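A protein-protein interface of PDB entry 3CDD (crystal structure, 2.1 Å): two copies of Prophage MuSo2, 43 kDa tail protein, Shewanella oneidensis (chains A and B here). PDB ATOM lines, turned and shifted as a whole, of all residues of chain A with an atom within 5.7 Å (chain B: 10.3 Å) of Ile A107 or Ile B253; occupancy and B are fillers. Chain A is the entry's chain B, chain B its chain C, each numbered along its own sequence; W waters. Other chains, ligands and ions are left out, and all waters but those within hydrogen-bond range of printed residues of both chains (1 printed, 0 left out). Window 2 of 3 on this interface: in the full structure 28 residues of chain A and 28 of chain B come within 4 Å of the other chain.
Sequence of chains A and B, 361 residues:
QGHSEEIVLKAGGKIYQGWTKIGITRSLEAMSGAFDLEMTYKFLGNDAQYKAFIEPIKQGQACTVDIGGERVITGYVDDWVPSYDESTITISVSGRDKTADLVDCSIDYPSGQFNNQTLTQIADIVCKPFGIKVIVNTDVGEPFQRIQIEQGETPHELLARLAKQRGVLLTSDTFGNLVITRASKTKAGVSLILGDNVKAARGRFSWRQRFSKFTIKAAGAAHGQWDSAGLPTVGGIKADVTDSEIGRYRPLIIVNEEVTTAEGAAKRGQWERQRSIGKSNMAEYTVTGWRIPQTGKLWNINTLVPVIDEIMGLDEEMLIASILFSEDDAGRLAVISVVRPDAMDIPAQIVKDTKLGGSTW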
ATOM      1  N   CYS A 105      28.559 -22.799  24.977  1.00  0.00           N
ATOM      2  CA  CYS A 105      27.286 -22.271  24.438  1.00  0.00           C
ATOM      3  C   CYS A 105      27.169 -20.748  24.427  1.00  0.00           C
ATOM      4  O   CYS A 105      27.856 -20.069  25.165  1.00  0.00           O
ATOM      5  CB  CYS A 105      26.096 -22.844  25.203  1.00  0.00           C
ATOM      6  SG  CYS A 105      26.034 -24.636  25.235  1.00  0.00           S
ATOM      7  N   SER A 106      26.271 -20.229  23.594  1.00  0.00           N
ATOM      8  CA  SER A 106      26.071 -18.791  23.458  1.00  0.00           C
ATOM      9  C   SER A 106      25.158 -18.231  24.540  1.00  0.00           C
ATOM     10  O   SER A 106      24.272 -18.933  25.044  1.00  0.00           O
ATOM     11  CB  SER A 106      25.484 -18.477  22.083  1.00  0.00           C
ATOM     12  OG  SER A 106      26.341 -18.934  21.057  1.00  0.00           O
ATOM     13  N   ILE A 107      25.385 -16.968  24.897  1.00  0.00           N
ATOM     14  CA  ILE A 107      24.470 -16.255  25.774  1.00  0.00           C
ATOM     15  C   ILE A 107      23.259 -15.879  24.942  1.00  0.00           C
ATOM     16  O   ILE A 107      23.380 -15.252  23.883  1.00  0.00           O
ATOM     17  CB  ILE A 107      25.076 -14.968  26.387  1.00  0.00           C
ATOM     18  CG1 ILE A 107      26.227 -15.301  27.329  1.00  0.00           C
ATOM     19  CG2 ILE A 107      24.005 -14.188  27.173  1.00  0.00           C
ATOM     20  CD1 ILE A 107      27.146 -14.135  27.603  1.00  0.00           C
ATOM     21  N   ASP A 108      22.097 -16.294  25.425  1.00  0.00           N
ATOM     22  CA  ASP A 108      20.831 -15.911  24.832  1.00  0.00           C
ATOM     23  C   ASP A 108      20.126 -14.976  25.805  1.00  0.00           C
ATOM     24  O   ASP A 108      19.503 -15.413  26.776  1.00  0.00           O
ATOM     25  CB  ASP A 108      19.982 -17.148  24.547  1.00  0.00           C
ATOM     26  CG  ASP A 108      18.618 -16.808  23.992  1.00  0.00           C
ATOM     27  OD1 ASP A 108      18.331 -15.610  23.738  1.00  0.00           O
ATOM     28  OD2 ASP A 108      17.823 -17.754  23.814  1.00  0.00           O
ATOM     29  N   TYR A 109      20.244 -13.682  25.545  1.00  0.00           N
ATOM     30  CA  TYR A 109      19.665 -12.676  26.418  1.00  0.00           C
ATOM     31  C   TYR A 109      19.162 -11.512  25.562  1.00  0.00           C
ATOM     32  O   TYR A 109      19.911 -10.570  25.287  1.00  0.00           O
ATOM     33  CB  TYR A 109      20.706 -12.242  27.453  1.00  0.00           C
ATOM     34  CG  TYR A 109      20.179 -11.361  28.556  1.00  0.00           C
ATOM     35  CD1 TYR A 109      19.334 -11.870  29.544  1.00  0.00           C
ATOM     36  CD2 TYR A 109      20.550 -10.023  28.627  1.00  0.00           C
ATOM     37  CE1 TYR A 109      18.858 -11.055  30.571  1.00  0.00           C
ATOM     38  CE2 TYR A 109      20.082  -9.199  29.641  1.00  0.00           C
ATOM     39  CZ  TYR A 109      19.239  -9.716  30.608  1.00  0.00           C
ATOM     40  OH  TYR A 109      18.780  -8.884  31.604  1.00  0.00           O
ATOM     41  N   PHE A 114      23.416  -5.449  30.220  1.00  0.00           N
ATOM     42  CA  PHE A 114      23.199  -5.393  31.659  1.00  0.00           C
ATOM     43  C   PHE A 114      23.491  -3.980  32.135  1.00  0.00           C
ATOM     44  O   PHE A 114      24.470  -3.350  31.661  1.00  0.00           O
ATOM     45  CB  PHE A 114      24.098  -6.409  32.370  1.00  0.00           C
ATOM     46  CG  PHE A 114      23.939  -7.814  31.858  1.00  0.00           C
ATOM     47  CD1 PHE A 114      24.802  -8.317  30.892  1.00  0.00           C
ATOM     48  CD2 PHE A 114      22.921  -8.632  32.336  1.00  0.00           C
ATOM     49  CE1 PHE A 114      24.652  -9.601  30.411  1.00  0.00           C
ATOM     50  CE2 PHE A 114      22.768  -9.930  31.861  1.00  0.00           C
ATOM     51  CZ  PHE A 114      23.633 -10.415  30.893  1.00  0.00           C
ATOM     52  N   VAL A 126      23.144 -15.225  33.469  1.00  0.00           N
ATOM     53  CA  VAL A 126      23.636 -16.035  32.345  1.00  0.00           C
ATOM     54  C   VAL A 126      23.726 -17.542  32.641  1.00  0.00           C
ATOM     55  O   VAL A 126      23.580 -18.354  31.722  1.00  0.00           O
ATOM     56  CB  VAL A 126      24.944 -15.472  31.697  1.00  0.00           C
ATOM     57  CG1 VAL A 126      24.750 -14.003  31.282  1.00  0.00           C
ATOM     58  CG2 VAL A 126      26.146 -15.624  32.613  1.00  0.00           C
ATOM     59  N   ILE A 149      26.530  -7.495  25.666  1.00  0.00           N
ATOM     60  CA  ILE A 149      26.911  -8.823  25.212  1.00  0.00           C
ATOM     61  C   ILE A 149      27.424  -8.723  23.773  1.00  0.00           C
ATOM     62  O   ILE A 149      26.733  -8.207  22.885  1.00  0.00           O
ATOM     63  CB  ILE A 149      25.751  -9.855  25.359  1.00  0.00           C
ATOM     64  CG1 ILE A 149      25.333  -9.970  26.829  1.00  0.00           C
ATOM     65  CG2 ILE A 149      26.173 -11.224  24.852  1.00  0.00           C
ATOM     66  CD1 ILE A 149      23.881 -10.318  27.024  1.00  0.00           C
ATOM     67  N   GLY A 152      27.742 -13.493  19.658  1.00  0.00           N
ATOM     68  CA  GLY A 152      28.064 -14.903  19.859  1.00  0.00           C
ATOM     69  C   GLY A 152      28.793 -15.189  21.157  1.00  0.00           C
ATOM     70  O   GLY A 152      29.273 -16.308  21.369  1.00  0.00           O
ATOM     71  N   GLU A 153      28.875 -14.188  22.031  1.00  0.00           N
ATOM     72  CA  GLU A 153      29.610 -14.319  23.294  1.00  0.00           C
ATOM     73  C   GLU A 153      29.015 -15.395  24.208  1.00  0.00           C
ATOM     74  O   GLU A 153      27.794 -15.524  24.329  1.00  0.00           O
ATOM     75  CB  GLU A 153      29.703 -12.976  24.022  1.00  0.00           C
ATOM     76  CG  GLU A 153      30.636 -13.002  25.233  1.00  0.00           C
ATOM     77  CD  GLU A 153      31.062 -11.625  25.687  1.00  0.00           C
ATOM     78  OE1 GLU A 153      30.180 -10.773  25.928  1.00  0.00           O
ATOM     79  OE2 GLU A 153      32.287 -11.396  25.812  1.00  0.00           O
ATOM     80  N   THR A 154      29.899 -16.180  24.816  1.00  0.00           N
ATOM     81  CA  THR A 154      29.515 -17.267  25.713  1.00  0.00           C
ATOM     82  C   THR A 154      29.444 -16.737  27.146  1.00  0.00           C
ATOM     83  O   THR A 154      30.019 -15.672  27.453  1.00  0.00           O
ATOM     84  CB  THR A 154      30.522 -18.439  25.660  1.00  0.00           C
ATOM     85  OG1 THR A 154      31.747 -18.052  26.295  1.00  0.00           O
ATOM     86  CG2 THR A 154      30.791 -18.884  24.227  1.00  0.00           C
ATOM     87  N   PRO A 155      28.719 -17.453  28.031  1.00  0.00           N
ATOM     88  CA  PRO A 155      28.712 -17.042  29.430  1.00  0.00           C
ATOM     89  C   PRO A 155      30.126 -16.966  29.996  1.00  0.00           C
ATOM     90  O   PRO A 155      30.444 -16.018  30.700  1.00  0.00           O
ATOM     91  CB  PRO A 155      27.917 -18.152  30.111  1.00  0.00           C
ATOM     92  CG  PRO A 155      27.021 -18.656  29.053  1.00  0.00           C
ATOM     93  CD  PRO A 155      27.841 -18.614  27.800  1.00  0.00           C
ATOM     94  N   LEU A 158      32.036 -13.743  28.673  1.00  0.00           N
ATOM     95  CA  LEU A 158      31.525 -12.522  29.317  1.00  0.00           C
ATOM     96  C   LEU A 158      32.009 -12.391  30.763  1.00  0.00           C
ATOM     97  O   LEU A 158      32.634 -11.389  31.140  1.00  0.00           O
ATOM     98  CB  LEU A 158      29.990 -12.455  29.251  1.00  0.00           C
ATOM     99  CG  LEU A 158      29.277 -11.348  30.065  1.00  0.00           C
ATOM    100  CD1 LEU A 158      29.493  -9.988  29.441  1.00  0.00           C
ATOM    101  CD2 LEU A 158      27.785 -11.627  30.208  1.00  0.00           C
ATOM    102  N   PHE B 211      24.489 -29.196  19.853  1.00  0.00           N
ATOM    103  CA  PHE B 211      23.741 -28.095  20.434  1.00  0.00           C
ATOM    104  C   PHE B 211      22.256 -28.369  20.305  1.00  0.00           C
ATOM    105  O   PHE B 211      21.836 -29.130  19.442  1.00  0.00           O
ATOM    106  CB  PHE B 211      24.151 -26.769  19.775  1.00  0.00           C
ATOM    107  CG  PHE B 211      25.578 -26.393  20.053  1.00  0.00           C
ATOM    108  CD1 PHE B 211      26.590 -26.747  19.175  1.00  0.00           C
ATOM    109  CD2 PHE B 211      25.916 -25.741  21.233  1.00  0.00           C
ATOM    110  CE1 PHE B 211      27.929 -26.429  19.457  1.00  0.00           C
ATOM    111  CE2 PHE B 211      27.228 -25.411  21.518  1.00  0.00           C
ATOM    112  CZ  PHE B 211      28.246 -25.763  20.632  1.00  0.00           C
ATOM    113  N   SER B 212      21.452 -27.773  21.168  1.00  0.00           N
ATOM    114  CA  SER B 212      20.020 -28.070  21.156  1.00  0.00           C
ATOM    115  C   SER B 212      19.297 -27.175  20.168  1.00  0.00           C
ATOM    116  O   SER B 212      18.294 -27.570  19.577  1.00  0.00           O
ATOM    117  CB  SER B 212      19.427 -27.907  22.548  1.00  0.00           C
ATOM    118  OG  SER B 212      19.761 -26.635  23.069  1.00  0.00           O
ATOM    119  N   LYS B 213      19.827 -25.966  19.995  1.00  0.00           N
ATOM    120  CA  LYS B 213      19.231 -24.967  19.128  1.00  0.00           C
ATOM    121  C   LYS B 213      20.318 -24.229  18.362  1.00  0.00           C
ATOM    122  O   LYS B 213      21.319 -23.765  18.946  1.00  0.00           O
ATOM    123  CB  LYS B 213      18.393 -23.992  19.958  1.00  0.00           C
ATOM    124  CG  LYS B 213      17.425 -23.140  19.145  1.00  0.00           C
ATOM    125  CD  LYS B 213      16.365 -22.489  20.035  1.00  0.00           C
ATOM    126  CE  LYS B 213      15.316 -23.506  20.519  1.00  0.00           C
ATOM    127  NZ  LYS B 213      14.058 -22.863  21.045  1.00  0.00           N
ATOM    128  N   PHE B 214      20.142 -24.155  17.047  1.00  0.00           N
ATOM    129  CA  PHE B 214      21.005 -23.339  16.200  1.00  0.00           C
ATOM    130  C   PHE B 214      20.249 -22.090  15.732  1.00  0.00           C
ATOM    131  O   PHE B 214      19.244 -22.194  15.025  1.00  0.00           O
ATOM    132  CB  PHE B 214      21.505 -24.154  15.004  1.00  0.00           C
ATOM    133  CG  PHE B 214      22.432 -25.284  15.377  1.00  0.00           C
ATOM    134  CD1 PHE B 214      21.927 -26.535  15.726  1.00  0.00           C
ATOM    135  CD2 PHE B 214      23.809 -25.102  15.364  1.00  0.00           C
ATOM    136  CE1 PHE B 214      22.780 -27.584  16.066  1.00  0.00           C
ATOM    137  CE2 PHE B 214      24.670 -26.163  15.693  1.00  0.00           C
ATOM    138  CZ  PHE B 214      24.151 -27.396  16.048  1.00  0.00           C
ATOM    139  N   THR B 215      20.716 -20.919  16.170  1.00  0.00           N
ATOM    140  CA  THR B 215      20.161 -19.623  15.745  1.00  0.00           C
ATOM    141  C   THR B 215      21.127 -18.954  14.764  1.00  0.00           C
ATOM    142  O   THR B 215      22.280 -18.672  15.115  1.00  0.00           O
ATOM    143  CB  THR B 215      19.912 -18.699  16.966  1.00  0.00           C
ATOM    144  OG1 THR B 215      18.945 -19.304  17.836  1.00  0.00           O
ATOM    145  CG2 THR B 215      19.385 -17.326  16.537  1.00  0.00           C
ATOM    146  N   ILE B 216      20.670 -18.734  13.533  1.00  0.00           N
ATOM    147  CA  ILE B 216      21.481 -18.057  12.516  1.00  0.00           C
ATOM    148  C   ILE B 216      20.943 -16.638  12.322  1.00  0.00           C
ATOM    149  O   ILE B 216      19.739 -16.462  12.126  1.00  0.00           O
ATOM    150  CB  ILE B 216      21.475 -18.826  11.161  1.00  0.00           C
ATOM    151  CG1 ILE B 216      21.944 -20.281  11.347  1.00  0.00           C
ATOM    152  CG2 ILE B 216      22.290 -18.078  10.077  1.00  0.00           C
ATOM    153  CD1 ILE B 216      23.427 -20.474  11.665  1.00  0.00           C
ATOM    154  N   LYS B 217      21.834 -15.646  12.379  1.00  0.00           N
ATOM    155  CA  LYS B 217      21.458 -14.227  12.280  1.00  0.00           C
ATOM    156  C   LYS B 217      22.225 -13.510  11.177  1.00  0.00           C
ATOM    157  O   LYS B 217      23.318 -13.932  10.790  1.00  0.00           O
ATOM    158  CB  LYS B 217      21.713 -13.497  13.606  1.00  0.00           C
ATOM    159  CG  LYS B 217      21.131 -14.161  14.837  1.00  0.00           C
ATOM    160  CD  LYS B 217      21.494 -13.421  16.128  1.00  0.00           C
ATOM    161  CE  LYS B 217      20.680 -12.132  16.333  1.00  0.00           C
ATOM    162  NZ  LYS B 217      21.485 -10.883  16.135  1.00  0.00           N
ATOM    163  N   ALA B 218      21.654 -12.415  10.678  1.00  0.00           N
ATOM    164  CA  ALA B 218      22.366 -11.492   9.788  1.00  0.00           C
ATOM    165  C   ALA B 218      23.362 -10.638  10.572  1.00  0.00           C
ATOM    166  O   ALA B 218      23.195 -10.421  11.779  1.00  0.00           O
ATOM    167  CB  ALA B 218      21.379 -10.604   9.044  1.00  0.00           C
ATOM    168  N   ILE B 237      16.888 -10.420  10.076  1.00  0.00           N
ATOM    169  CA  ILE B 237      16.890 -11.748   9.486  1.00  0.00           C
ATOM    170  C   ILE B 237      17.435 -12.758  10.498  1.00  0.00           C
ATOM    171  O   ILE B 237      18.542 -12.598  11.028  1.00  0.00           O
ATOM    172  CB  ILE B 237      17.667 -11.776   8.131  1.00  0.00           C
ATOM    173  CG1 ILE B 237      16.965 -10.899   7.080  1.00  0.00           C
ATOM    174  CG2 ILE B 237      17.894 -13.214   7.634  1.00  0.00           C
ATOM    175  CD1 ILE B 237      15.438 -11.085   6.995  1.00  0.00           C
ATOM    176  N   LYS B 238      16.626 -13.778  10.773  1.00  0.00           N
ATOM    177  CA  LYS B 238      16.894 -14.731  11.840  1.00  0.00           C
ATOM    178  C   LYS B 238      16.175 -16.039  11.515  1.00  0.00           C
ATOM    179  O   LYS B 238      15.120 -16.017  10.876  1.00  0.00           O
ATOM    180  CB  LYS B 238      16.367 -14.162  13.160  1.00  0.00           C
ATOM    181  CG  LYS B 238      16.872 -14.856  14.405  1.00  0.00           C
ATOM    182  CD  LYS B 238      15.972 -14.579  15.613  1.00  0.00           C
ATOM    183  CE  LYS B 238      16.390 -15.479  16.780  1.00  0.00           C
ATOM    184  NZ  LYS B 238      15.396 -15.556  17.903  1.00  0.00           N
ATOM    185  N   ALA B 239      16.757 -17.166  11.931  1.00  0.00           N
ATOM    186  CA  ALA B 239      16.074 -18.468  11.928  1.00  0.00           C
ATOM    187  C   ALA B 239      16.618 -19.369  13.029  1.00  0.00           C
ATOM    188  O   ALA B 239      17.821 -19.405  13.258  1.00  0.00           O
ATOM    189  CB  ALA B 239      16.203 -19.155  10.587  1.00  0.00           C
ATOM    190  N   ASP B 240      15.711 -20.074  13.709  1.00  0.00           N
ATOM    191  CA  ASP B 240      16.062 -21.107  14.680  1.00  0.00           C
ATOM    192  C   ASP B 240      15.868 -22.475  14.053  1.00  0.00           C
ATOM    193  O   ASP B 240      14.917 -22.699  13.284  1.00  0.00           O
ATOM    194  CB  ASP B 240      15.212 -21.007  15.950  1.00  0.00           C
ATOM    195  CG  ASP B 240      15.466 -19.728  16.734  1.00  0.00           C
ATOM    196  OD1 ASP B 240      15.797 -19.823  17.933  1.00  0.00           O
ATOM    197  OD2 ASP B 240      15.321 -18.622  16.170  1.00  0.00           O
ATOM    198  N   VAL B 241      16.792 -23.371  14.389  1.00  0.00           N
ATOM    199  CA  VAL B 241      16.794 -24.754  13.941  1.00  0.00           C
ATOM    200  C   VAL B 241      17.161 -25.601  15.153  1.00  0.00           C
ATOM    201  O   VAL B 241      18.245 -25.448  15.716  1.00  0.00           O
ATOM    202  CB  VAL B 241      17.821 -24.969  12.797  1.00  0.00           C
ATOM    203  CG1 VAL B 241      18.009 -26.445  12.503  1.00  0.00           C
ATOM    204  CG2 VAL B 241      17.389 -24.198  11.529  1.00  0.00           C
ATOM    205  N   TYR B 249      19.565 -27.887  27.502  1.00  0.00           N
ATOM    206  CA  TYR B 249      19.690 -26.518  27.019  1.00  0.00           C
ATOM    207  C   TYR B 249      21.140 -26.234  26.637  1.00  0.00           C
ATOM    208  O   TYR B 249      22.005 -26.039  27.496  1.00  0.00           O
ATOM    209  CB  TYR B 249      19.185 -25.526  28.080  1.00  0.00           C
ATOM    210  CG  TYR B 249      19.341 -24.068  27.714  1.00  0.00           C
ATOM    211  CD1 TYR B 249      18.367 -23.394  26.956  1.00  0.00           C
ATOM    212  CD2 TYR B 249      20.447 -23.348  28.150  1.00  0.00           C
ATOM    213  CE1 TYR B 249      18.519 -22.050  26.627  1.00  0.00           C
ATOM    214  CE2 TYR B 249      20.614 -22.010  27.832  1.00  0.00           C
ATOM    215  CZ  TYR B 249      19.649 -21.365  27.071  1.00  0.00           C
ATOM    216  OH  TYR B 249      19.844 -20.038  26.769  1.00  0.00           O
ATOM    217  N   ARG B 250      21.389 -26.236  25.332  1.00  0.00           N
ATOM    218  CA  ARG B 250      22.700 -25.941  24.767  1.00  0.00           C
ATOM    219  C   ARG B 250      22.495 -25.157  23.466  1.00  0.00           C
ATOM    220  O   ARG B 250      22.483 -25.763  22.389  1.00  0.00           O
ATOM    221  CB  ARG B 250      23.472 -27.242  24.499  1.00  0.00           C
ATOM    222  CG  ARG B 250      24.204 -27.825  25.713  1.00  0.00           C
ATOM    223  CD  ARG B 250      24.923 -29.150  25.387  1.00  0.00           C
ATOM    224  NE  ARG B 250      25.936 -29.021  24.337  1.00  0.00           N
ATOM    225  CZ  ARG B 250      27.184 -28.599  24.533  1.00  0.00           C
ATOM    226  NH1 ARG B 250      27.598 -28.272  25.748  1.00  0.00           N
ATOM    227  NH2 ARG B 250      28.028 -28.514  23.512  1.00  0.00           N
ATOM    228  N   PRO B 251      22.277 -23.817  23.567  1.00  0.00           N
ATOM    229  CA  PRO B 251      22.039 -22.983  22.396  1.00  0.00           C
ATOM    230  C   PRO B 251      23.309 -22.461  21.745  1.00  0.00           C
ATOM    231  O   PRO B 251      24.293 -22.157  22.430  1.00  0.00           O
ATOM    232  CB  PRO B 251      21.236 -21.802  22.969  1.00  0.00           C
ATOM    233  CG  PRO B 251      21.772 -21.653  24.359  1.00  0.00           C
ATOM    234  CD  PRO B 251      22.214 -23.030  24.814  1.00  0.00           C
ATOM    235  N   LEU B 252      23.283 -22.354  20.418  1.00  0.00           N
ATOM    236  CA  LEU B 252      24.372 -21.687  19.693  1.00  0.00           C
ATOM    237  C   LEU B 252      23.822 -20.652  18.718  1.00  0.00           C
ATOM    238  O   LEU B 252      22.928 -20.923  17.906  1.00  0.00           O
ATOM    239  CB  LEU B 252      25.303 -22.692  18.991  1.00  0.00           C
ATOM    240  CG  LEU B 252      26.608 -22.146  18.414  1.00  0.00           C
ATOM    241  CD1 LEU B 252      27.603 -21.766  19.511  1.00  0.00           C
ATOM    242  CD2 LEU B 252      27.240 -23.188  17.469  1.00  0.00           C
ATOM    243  N   ILE B 253      24.364 -19.447  18.825  1.00  0.00           N
ATOM    244  CA  ILE B 253      23.939 -18.339  17.990  1.00  0.00           C
ATOM    245  C   ILE B 253      25.110 -17.988  17.080  1.00  0.00           C
ATOM    246  O   ILE B 253      26.234 -17.827  17.555  1.00  0.00           O
ATOM    247  CB  ILE B 253      23.519 -17.123  18.845  1.00  0.00           C
ATOM    248  CG1 ILE B 253      22.333 -17.504  19.745  1.00  0.00           C
ATOM    249  CG2 ILE B 253      23.146 -15.947  17.934  1.00  0.00           C
ATOM    250  CD1 ILE B 253      22.132 -16.610  20.973  1.00  0.00           C
ATOM    251  N   ILE B 254      24.838 -17.908  15.776  1.00  0.00           N
ATOM    252  CA  ILE B 254      25.862 -17.707  14.753  1.00  0.00           C
ATOM    253  C   ILE B 254      25.434 -16.580  13.817  1.00  0.00           C
ATOM    254  O   ILE B 254      24.328 -16.611  13.268  1.00  0.00           O
ATOM    255  CB  ILE B 254      26.111 -19.021  13.941  1.00  0.00           C
ATOM    256  CG1 ILE B 254      26.620 -20.139  14.861  1.00  0.00           C
ATOM    257  CG2 ILE B 254      27.086 -18.782  12.805  1.00  0.00           C
ATOM    258  CD1 ILE B 254      26.559 -21.534  14.265  1.00  0.00           C
ATOM    259  N   VAL B 255      26.305 -15.583  13.652  1.00  0.00           N
ATOM    260  CA  VAL B 255      26.034 -14.471  12.741  1.00  0.00           C
ATOM    261  C   VAL B 255      26.638 -14.713  11.363  1.00  0.00           C
ATOM    262  O   VAL B 255      27.845 -14.572  11.178  1.00  0.00           O
ATOM    263  CB  VAL B 255      26.502 -13.096  13.305  1.00  0.00           C
ATOM    264  CG1 VAL B 255      25.715 -12.742  14.556  1.00  0.00           C
ATOM    265  CG2 VAL B 255      28.005 -13.092  13.593  1.00  0.00           C
ATOM    266  N   ASN B 256      25.798 -15.098  10.404  1.00  0.00           N
ATOM    267  CA  ASN B 256      26.233 -15.252   9.016  1.00  0.00           C
ATOM    268  C   ASN B 256      25.930 -13.973   8.237  1.00  0.00           C
ATOM    269  O   ASN B 256      24.766 -13.575   8.094  1.00  0.00           O
ATOM    270  CB  ASN B 256      25.573 -16.478   8.378  1.00  0.00           C
ATOM    271  CG  ASN B 256      26.368 -17.033   7.213  1.00  0.00           C
ATOM    272  OD1 ASN B 256      26.395 -16.454   6.129  1.00  0.00           O
ATOM    273  ND2 ASN B 256      27.017 -18.164   7.431  1.00  0.00           N
ATOM    274  N   ARG B 268      20.808 -22.422   6.153  1.00  0.00           N
ATOM    275  CA  ARG B 268      22.099 -22.341   6.828  1.00  0.00           C
ATOM    276  C   ARG B 268      22.055 -23.066   8.185  1.00  0.00           C
ATOM    277  O   ARG B 268      22.974 -23.813   8.522  1.00  0.00           O
ATOM    278  CB  ARG B 268      22.513 -20.874   6.999  1.00  0.00           C
ATOM    279  CG  ARG B 268      23.856 -20.651   7.670  1.00  0.00           C
ATOM    280  CD  ARG B 268      25.007 -21.100   6.795  1.00  0.00           C
ATOM    281  NE  ARG B 268      26.215 -21.380   7.573  1.00  0.00           N
ATOM    282  CZ  ARG B 268      27.408 -21.647   7.044  1.00  0.00           C
ATOM    283  NH1 ARG B 268      27.577 -21.673   5.727  1.00  0.00           N
ATOM    284  NH2 ARG B 268      28.440 -21.891   7.841  1.00  0.00           N
ATOM    285  N   GLY B 269      20.980 -22.846   8.948  1.00  0.00           N
ATOM    286  CA  GLY B 269      20.793 -23.493  10.254  1.00  0.00           C
ATOM    287  C   GLY B 269      20.842 -25.014  10.209  1.00  0.00           C
ATOM    288  O   GLY B 269      21.577 -25.644  10.973  1.00  0.00           O
ATOM    289  N   GLU B 272      24.149 -26.294   9.455  1.00  0.00           N
ATOM    290  CA  GLU B 272      24.973 -26.198  10.648  1.00  0.00           C
ATOM    291  C   GLU B 272      24.712 -27.374  11.590  1.00  0.00           C
ATOM    292  O   GLU B 272      25.658 -27.948  12.150  1.00  0.00           O
ATOM    293  CB  GLU B 272      24.729 -24.857  11.350  1.00  0.00           C
ATOM    294  CG  GLU B 272      25.957 -24.280  12.023  1.00  0.00           C
ATOM    295  CD  GLU B 272      27.055 -23.896  11.047  1.00  0.00           C
ATOM    296  OE1 GLU B 272      26.787 -23.143  10.086  1.00  0.00           O
ATOM    297  OE2 GLU B 272      28.197 -24.338  11.257  1.00  0.00           O
HETATM  298  O   HOH W   1      22.083 -18.688  26.936  1.00  0.00           O
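N of Ser A106 sits at hydrogen-bond distance from O of Pro B251 (3.0 Å). The backbone NH of Ile B253 sits at hydrogen-bond distance from the side-chain hydroxyl of Ser A106 (3.0 Å).
N of Ile A107 lies within hydrogen-bond range of O of Glu A153, at 2.9 Å. The backbone NH of Leu B252 lies within hydrogen-bond range of the backbone carbonyl oxygen of Lys B213 (2.8 Å). O of Leu B252 sits at hydrogen-bond distance from N of Thr B215, 2.8 Å away. N of Ser B212 is in hydrogen-bond range of O of Arg B250.
Among the printed residues, merely in contact across the chains: Cys A105 with Phe B211, Cys A105 with Arg B250, Cys A105 with Pro B251, Ser A106 with Leu B252, Ile A107 with Ile B253 and Asp A108 with Tyr B249.
Of chain B, only Ile B253 comes within 4 Å of Ile A107. Of chain A, only Ser A106 (3.0 Å) and Ile A107 (3.4 Å) come within 4 Å of Ile B253. Gly A152 touches none of the printed residues of chain B. No residue of chain B comes within 4 Å of Glu A153. No residue of chain B comes within 4 Å of Thr A154. Printed residues of chain A within 4 Å of Leu B252: Ser A106 (3.5 Å). Printed residues of chain B within 4 Å of Cys A105: Phe B211 (3.98 Å), Arg B250 (3.6 Å) and Pro B251 (3.4 Å). Of the printed residues of chain A, Arg B250 touches Cys A105 (3.6 Å). Ile B254 touches none of the printed residues of chain A. The nearest printed residue of chain A that does not touch Leu B252 is Cys A105 (5.0 Å).
Of the 24 printed residues of chain B, 6 touch a printed residue of chain A. Hydrophobic or aromatic side chains of chain B within 4 Å of the printed part of chain A: Phe B211, Tyr B249, Pro B251, Leu B252 and Ile B253. Of the 13 printed residues of chain A, 4 touch a printed residue of chain B. Among the printed residues, 8 pairs touch across the chains. Among the printed residues, no Asp or Glu carboxylate lies within 4 Å of a Lys or Arg side-chain nitrogen of the other chain.
No position is printed for both chains.
Water W1 lies within hydrogen-bond range of the side-chain hydroxyl of Tyr B249 (2.6 Å), the backbone NH of Asp A108 (2.8 Å) and the backbone carbonyl oxygen of Ser A106 (2.9 Å).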
